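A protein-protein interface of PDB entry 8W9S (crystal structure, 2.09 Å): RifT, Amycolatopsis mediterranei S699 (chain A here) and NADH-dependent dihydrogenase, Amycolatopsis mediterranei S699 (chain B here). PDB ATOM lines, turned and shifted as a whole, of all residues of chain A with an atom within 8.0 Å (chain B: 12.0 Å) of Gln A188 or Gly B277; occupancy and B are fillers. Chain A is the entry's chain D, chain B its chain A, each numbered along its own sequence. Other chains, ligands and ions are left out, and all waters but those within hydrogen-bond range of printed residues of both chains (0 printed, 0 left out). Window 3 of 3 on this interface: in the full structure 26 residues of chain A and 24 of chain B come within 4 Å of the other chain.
Printed residues of chain A that touch a printed residue of chain B: Gly A95, Gln A188, Gly A189, Ser A190 and Val A191. Hydrophobic or aromatic side chains of chain A that line the printed part of chain B: Val A191. Of the 10 printed residues of chain B, 8 touch a printed residue of chain A. Among the printed residues, 9 pairs touch across the chains.
No residue of chain B comes within 4 Å of Gly A94. Of chain B, only Ala B279 (3.1 Å), Asn B281 (3.5 Å) and Phe B282 (3.98 Å) come within 4 Å of Gly A95. No residue of chain B comes within 4 Å of Gly A97. Thr A100 touches none of the printed residues of chain B. No residue of chain B comes within 4 Å of Asp A187. Gln A188 touches just one residue of chain B: Gly B277. Of the printed residues of chain B, Gly A189 touches Asp B276. Printed residues of chain B within 4 Å of Val A191: Arg B273. Of the printed residues of chain A, Arg B273 touches Val A191 (3.3 Å). Of the printed residues of chain A, Val B274 touches Ser A190 (3.7 Å). Of chain A, only Gln A188 (3.5 Å) comes within 4 Å of Gly B277. Gly B280 touches none of the printed residues of chain A. The nearest residue of chain B that does not touch Gln A188 is Asp B276 (4.6 Å).
O of Ile A96 sits at hydrogen-bond distance from N of Gln A188, 2.9 Å away. The backbone carbonyl oxygen (O) of Ile A96 sits at hydrogen-bond distance from the backbone NH (N) of Gly A189.
O of Asp B276 sits at hydrogen-bond distance from N of Ser A190 (3.2 Å). The backbone carbonyl oxygen (O) of Ser A190 sits at hydrogen-bond distance from the backbone NH (N) of Val B275 (2.9 Å).
Among the printed residues, pairs that only touch across the chains: Gly A95 with Ala B279, Val A191 with Arg B273, Gly A189 with Asp B276, Gly A95 with Asn B281, Gln A188 with Gly B277, Ser A190 with Val B274 and Gly A95 with Phe B282.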
ATOM      1  N   GLY A  94      17.733  19.638 -10.637  1.00  0.00           N
ATOM      2  CA  GLY A  94      16.334  19.491 -10.272  1.00  0.00           C
ATOM      3  C   GLY A  94      15.706  18.155 -10.605  1.00  0.00           C
ATOM      4  O   GLY A  94      14.473  18.057 -10.629  1.00  0.00           O
ATOM      5  N   GLY A  95      16.510  17.115 -10.852  1.00  0.00           N
ATOM      6  CA  GLY A  95      15.949  15.827 -11.240  1.00  0.00           C
ATOM      7  C   GLY A  95      15.049  15.189 -10.192  1.00  0.00           C
ATOM      8  O   GLY A  95      14.167  14.403 -10.534  1.00  0.00           O
ATOM      9  N   ILE A  96      15.257  15.503  -8.910  1.00  0.00           N
ATOM     10  CA  ILE A  96      14.425  14.968  -7.833  1.00  0.00           C
ATOM     11  C   ILE A  96      13.640  16.063  -7.116  1.00  0.00           C
ATOM     12  O   ILE A  96      13.082  15.822  -6.034  1.00  0.00           O
ATOM     13  CB  ILE A  96      15.256  14.148  -6.821  1.00  0.00           C
ATOM     14  CG1 ILE A  96      16.302  15.022  -6.130  1.00  0.00           C
ATOM     15  CG2 ILE A  96      15.926  12.948  -7.479  1.00  0.00           C
ATOM     16  CD1 ILE A  96      17.054  14.307  -5.036  1.00  0.00           C
ATOM     17  N   GLY A  97      13.585  17.260  -7.690  1.00  0.00           N
ATOM     18  CA  GLY A  97      12.971  18.383  -7.012  1.00  0.00           C
ATOM     19  C   GLY A  97      13.865  18.919  -5.903  1.00  0.00           C
ATOM     20  O   GLY A  97      15.090  18.770  -5.924  1.00  0.00           O
ATOM     21  N   GLU A  98      13.240  19.560  -4.928  1.00  0.00           N
ATOM     22  CA  GLU A  98      13.980  20.092  -3.793  1.00  0.00           C
ATOM     23  C   GLU A  98      14.480  18.949  -2.909  1.00  0.00           C
ATOM     24  O   GLU A  98      13.685  18.127  -2.455  1.00  0.00           O
ATOM     25  CB  GLU A  98      13.096  21.034  -2.983  1.00  0.00           C
ATOM     26  CG  GLU A  98      13.808  21.581  -1.753  1.00  0.00           C
ATOM     27  CD  GLU A  98      12.952  22.549  -0.941  1.00  0.00           C
ATOM     28  OE1 GLU A  98      11.839  22.166  -0.513  1.00  0.00           O
ATOM     29  OE2 GLU A  98      13.395  23.699  -0.740  1.00  0.00           O
ATOM     30  N   LEU A  99      15.789  18.916  -2.657  1.00  0.00           N
ATOM     31  CA  LEU A  99      16.404  17.874  -1.843  1.00  0.00           C
ATOM     32  C   LEU A  99      16.016  18.004  -0.360  1.00  0.00           C
ATOM     33  O   LEU A  99      16.169  19.068   0.242  1.00  0.00           O
ATOM     34  CB  LEU A  99      17.921  17.959  -2.003  1.00  0.00           C
ATOM     35  CG  LEU A  99      18.757  17.023  -1.118  1.00  0.00           C
ATOM     36  CD1 LEU A  99      18.682  15.552  -1.623  1.00  0.00           C
ATOM     37  CD2 LEU A  99      20.212  17.526  -1.044  1.00  0.00           C
ATOM     38  N   THR A 100      15.516  16.922   0.241  1.00  0.00           N
ATOM     39  CA  THR A 100      15.155  16.967   1.660  1.00  0.00           C
ATOM     40  C   THR A 100      15.911  15.993   2.550  1.00  0.00           C
ATOM     41  O   THR A 100      16.114  16.291   3.729  1.00  0.00           O
ATOM     42  CB  THR A 100      13.651  16.714   1.856  1.00  0.00           C
ATOM     43  OG1 THR A 100      13.333  15.335   1.590  1.00  0.00           O
ATOM     44  CG2 THR A 100      12.834  17.635   0.957  1.00  0.00           C
ATOM     45  N   ILE A 185      16.702  11.807  -1.390  1.00  0.00           N
ATOM     46  CA  ILE A 185      15.261  11.987  -1.527  1.00  0.00           C
ATOM     47  C   ILE A 185      14.967  13.469  -1.677  1.00  0.00           C
ATOM     48  O   ILE A 185      15.395  14.283  -0.847  1.00  0.00           O
ATOM     49  CB  ILE A 185      14.497  11.414  -0.319  1.00  0.00           C
ATOM     50  CG1 ILE A 185      14.591   9.883  -0.282  1.00  0.00           C
ATOM     51  CG2 ILE A 185      13.032  11.883  -0.346  1.00  0.00           C
ATOM     52  CD1 ILE A 185      14.488   9.335   1.126  1.00  0.00           C
ATOM     53  N   GLY A 186      14.228  13.816  -2.729  1.00  0.00           N
ATOM     54  CA  GLY A 186      13.711  15.151  -2.919  1.00  0.00           C
ATOM     55  C   GLY A 186      12.194  15.113  -2.964  1.00  0.00           C
ATOM     56  O   GLY A 186      11.574  14.049  -2.897  1.00  0.00           O
ATOM     57  N   ASP A 187      11.599  16.294  -3.112  1.00  0.00           N
ATOM     58  CA  ASP A 187      10.145  16.310  -3.049  1.00  0.00           C
ATOM     59  C   ASP A 187       9.484  15.899  -4.361  1.00  0.00           C
ATOM     60  O   ASP A 187       8.252  15.884  -4.430  1.00  0.00           O
ATOM     61  CB  ASP A 187       9.644  17.679  -2.570  1.00  0.00           C
ATOM     62  CG  ASP A 187       9.894  18.805  -3.566  1.00  0.00           C
ATOM     63  OD1 ASP A 187      10.623  18.621  -4.569  1.00  0.00           O
ATOM     64  OD2 ASP A 187       9.371  19.911  -3.302  1.00  0.00           O
ATOM     65  N   GLN A 188      10.264  15.519  -5.382  1.00  0.00           N
ATOM     66  CA  GLN A 188       9.707  14.980  -6.616  1.00  0.00           C
ATOM     67  C   GLN A 188      10.270  13.614  -6.992  1.00  0.00           C
ATOM     68  O   GLN A 188       9.861  13.061  -8.018  1.00  0.00           O
ATOM     69  CB  GLN A 188       9.903  15.978  -7.778  1.00  0.00           C
ATOM     70  CG  GLN A 188       8.847  17.099  -7.722  1.00  0.00           C
ATOM     71  CD  GLN A 188       9.015  18.175  -8.780  1.00  0.00           C
ATOM     72  OE1 GLN A 188      10.075  18.804  -8.888  1.00  0.00           O
ATOM     73  NE2 GLN A 188       7.957  18.417  -9.551  1.00  0.00           N
ATOM     74  N   GLY A 189      11.161  13.044  -6.191  1.00  0.00           N
ATOM     75  CA  GLY A 189      11.675  11.721  -6.491  1.00  0.00           C
ATOM     76  C   GLY A 189      12.843  11.371  -5.595  1.00  0.00           C
ATOM     77  O   GLY A 189      13.212  12.118  -4.675  1.00  0.00           O
ATOM     78  N   SER A 190      13.417  10.198  -5.868  1.00  0.00           N
ATOM     79  CA  SER A 190      14.605   9.769  -5.161  1.00  0.00           C
ATOM     80  C   SER A 190      15.504   9.003  -6.113  1.00  0.00           C
ATOM     81  O   SER A 190      15.034   8.321  -7.029  1.00  0.00           O
ATOM     82  CB  SER A 190      14.268   8.906  -3.920  1.00  0.00           C
ATOM     83  OG  SER A 190      13.753   7.637  -4.290  1.00  0.00           O
ATOM     84  N   VAL A 191      16.807   9.120  -5.880  1.00  0.00           N
ATOM     85  CA  VAL A 191      17.814   8.445  -6.691  1.00  0.00           C
ATOM     86  C   VAL A 191      18.851   7.845  -5.757  1.00  0.00           C
ATOM     87  O   VAL A 191      19.184   8.438  -4.723  1.00  0.00           O
ATOM     88  CB  VAL A 191      18.481   9.411  -7.686  1.00  0.00           C
ATOM     89  CG1 VAL A 191      19.076  10.592  -6.941  1.00  0.00           C
ATOM     90  CG2 VAL A 191      19.549   8.679  -8.510  1.00  0.00           C
ATOM     91  N   ARG B 273      20.626   4.607  -9.744  1.00  0.00           N
ATOM     92  CA  ARG B 273      19.274   4.064  -9.815  1.00  0.00           C
ATOM     93  C   ARG B 273      18.259   5.106  -9.366  1.00  0.00           C
ATOM     94  O   ARG B 273      18.276   5.542  -8.207  1.00  0.00           O
ATOM     95  CB  ARG B 273      19.162   2.798  -8.956  1.00  0.00           C
ATOM     96  CG  ARG B 273      17.774   2.181  -8.932  1.00  0.00           C
ATOM     97  CD  ARG B 273      17.657   1.198  -7.742  1.00  0.00           C
ATOM     98  NE  ARG B 273      16.304   0.668  -7.592  1.00  0.00           N
ATOM     99  CZ  ARG B 273      15.948  -0.214  -6.666  1.00  0.00           C
ATOM    100  NH1 ARG B 273      16.852  -0.668  -5.804  1.00  0.00           N
ATOM    101  NH2 ARG B 273      14.692  -0.631  -6.604  1.00  0.00           N
ATOM    102  N   VAL B 274      17.375   5.498 -10.279  1.00  0.00           N
ATOM    103  CA  VAL B 274      16.225   6.324  -9.927  1.00  0.00           C
ATOM    104  C   VAL B 274      15.205   5.400  -9.274  1.00  0.00           C
ATOM    105  O   VAL B 274      14.697   4.475  -9.909  1.00  0.00           O
ATOM    106  CB  VAL B 274      15.632   7.033 -11.147  1.00  0.00           C
ATOM    107  CG1 VAL B 274      14.429   7.868 -10.735  1.00  0.00           C
ATOM    108  CG2 VAL B 274      16.680   7.898 -11.840  1.00  0.00           C
ATOM    109  N   VAL B 275      14.922   5.627  -7.999  1.00  0.00           N
ATOM    110  CA  VAL B 275      14.050   4.705  -7.282  1.00  0.00           C
ATOM    111  C   VAL B 275      12.589   5.086  -7.455  1.00  0.00           C
ATOM    112  O   VAL B 275      11.742   4.211  -7.635  1.00  0.00           O
ATOM    113  CB  VAL B 275      14.466   4.626  -5.797  1.00  0.00           C
ATOM    114  CG1 VAL B 275      13.535   3.692  -5.021  1.00  0.00           C
ATOM    115  CG2 VAL B 275      15.891   4.120  -5.697  1.00  0.00           C
ATOM    116  N   ASP B 276      12.267   6.382  -7.454  1.00  0.00           N
ATOM    117  CA  ASP B 276      10.893   6.807  -7.687  1.00  0.00           C
ATOM    118  C   ASP B 276      10.859   8.192  -8.320  1.00  0.00           C
ATOM    119  O   ASP B 276      11.847   8.930  -8.304  1.00  0.00           O
ATOM    120  CB  ASP B 276      10.086   6.805  -6.394  1.00  0.00           C
ATOM    121  CG  ASP B 276      10.769   7.576  -5.289  1.00  0.00           C
ATOM    122  OD1 ASP B 276      10.495   8.784  -5.159  1.00  0.00           O
ATOM    123  OD2 ASP B 276      11.593   6.970  -4.559  1.00  0.00           O
ATOM    124  N   GLY B 277       9.695   8.540  -8.877  1.00  0.00           N
ATOM    125  CA  GLY B 277       9.485   9.850  -9.452  1.00  0.00           C
ATOM    126  C   GLY B 277       9.763   9.949 -10.935  1.00  0.00           C
ATOM    127  O   GLY B 277       9.213  10.836 -11.600  1.00  0.00           O
ATOM    128  N   GLY B 278      10.606   9.079 -11.472  1.00  0.00           N
ATOM    129  CA  GLY B 278      10.697   8.952 -12.910  1.00  0.00           C
ATOM    130  C   GLY B 278      11.638   9.909 -13.596  1.00  0.00           C
ATOM    131  O   GLY B 278      11.514  10.113 -14.809  1.00  0.00           O
ATOM    132  N   ALA B 279      12.583  10.500 -12.866  1.00  0.00           N
ATOM    133  CA  ALA B 279      13.515  11.432 -13.482  1.00  0.00           C
ATOM    134  C   ALA B 279      14.268  10.763 -14.628  1.00  0.00           C
ATOM    135  O   ALA B 279      14.544   9.556 -14.606  1.00  0.00           O
ATOM    136  CB  ALA B 279      14.503  11.964 -12.450  1.00  0.00           C
ATOM    137  N   GLY B 280      14.592  11.567 -15.645  1.00  0.00           N
ATOM    138  CA  GLY B 280      15.268  11.064 -16.823  1.00  0.00           C
ATOM    139  C   GLY B 280      16.677  11.587 -17.015  1.00  0.00           C
ATOM    140  O   GLY B 280      17.328  11.243 -18.005  1.00  0.00           O
ATOM    141  N   ASN B 281      17.177  12.402 -16.085  1.00  0.00           N
ATOM    142  CA  ASN B 281      18.479  13.033 -16.259  1.00  0.00           C
ATOM    143  C   ASN B 281      19.575  12.368 -15.435  1.00  0.00           C
ATOM    144  O   ASN B 281      20.559  13.030 -15.073  1.00  0.00           O
ATOM    145  CB  ASN B 281      18.402  14.522 -15.925  1.00  0.00           C
ATOM    146  CG  ASN B 281      17.897  14.775 -14.521  1.00  0.00           C
ATOM    147  OD1 ASN B 281      17.021  14.052 -14.028  1.00  0.00           O
ATOM    148  ND2 ASN B 281      18.432  15.818 -13.870  1.00  0.00           N
ATOM    149  N   PHE B 282      19.449  11.062 -15.164  1.00  0.00           N
ATOM    150  CA  PHE B 282      20.440  10.319 -14.390  1.00  0.00           C
ATOM    151  C   PHE B 282      21.034   9.167 -15.196  1.00  0.00           C
ATOM    152  O   PHE B 282      21.397   8.125 -14.639  1.00  0.00           O
ATOM    153  CB  PHE B 282      19.839   9.805 -13.084  1.00  0.00           C
ATOM    154  CG  PHE B 282      19.515  10.892 -12.107  1.00  0.00           C
ATOM    155  CD1 PHE B 282      18.211  11.356 -11.978  1.00  0.00           C
ATOM    156  CD2 PHE B 282      20.505  11.454 -11.318  1.00  0.00           C
ATOM    157  CE1 PHE B 282      17.903  12.365 -11.065  1.00  0.00           C
ATOM    158  CE2 PHE B 282      20.204  12.452 -10.404  1.00  0.00           C
ATOM    159  CZ  PHE B 282      18.901  12.915 -10.281  1.00  0.00           C
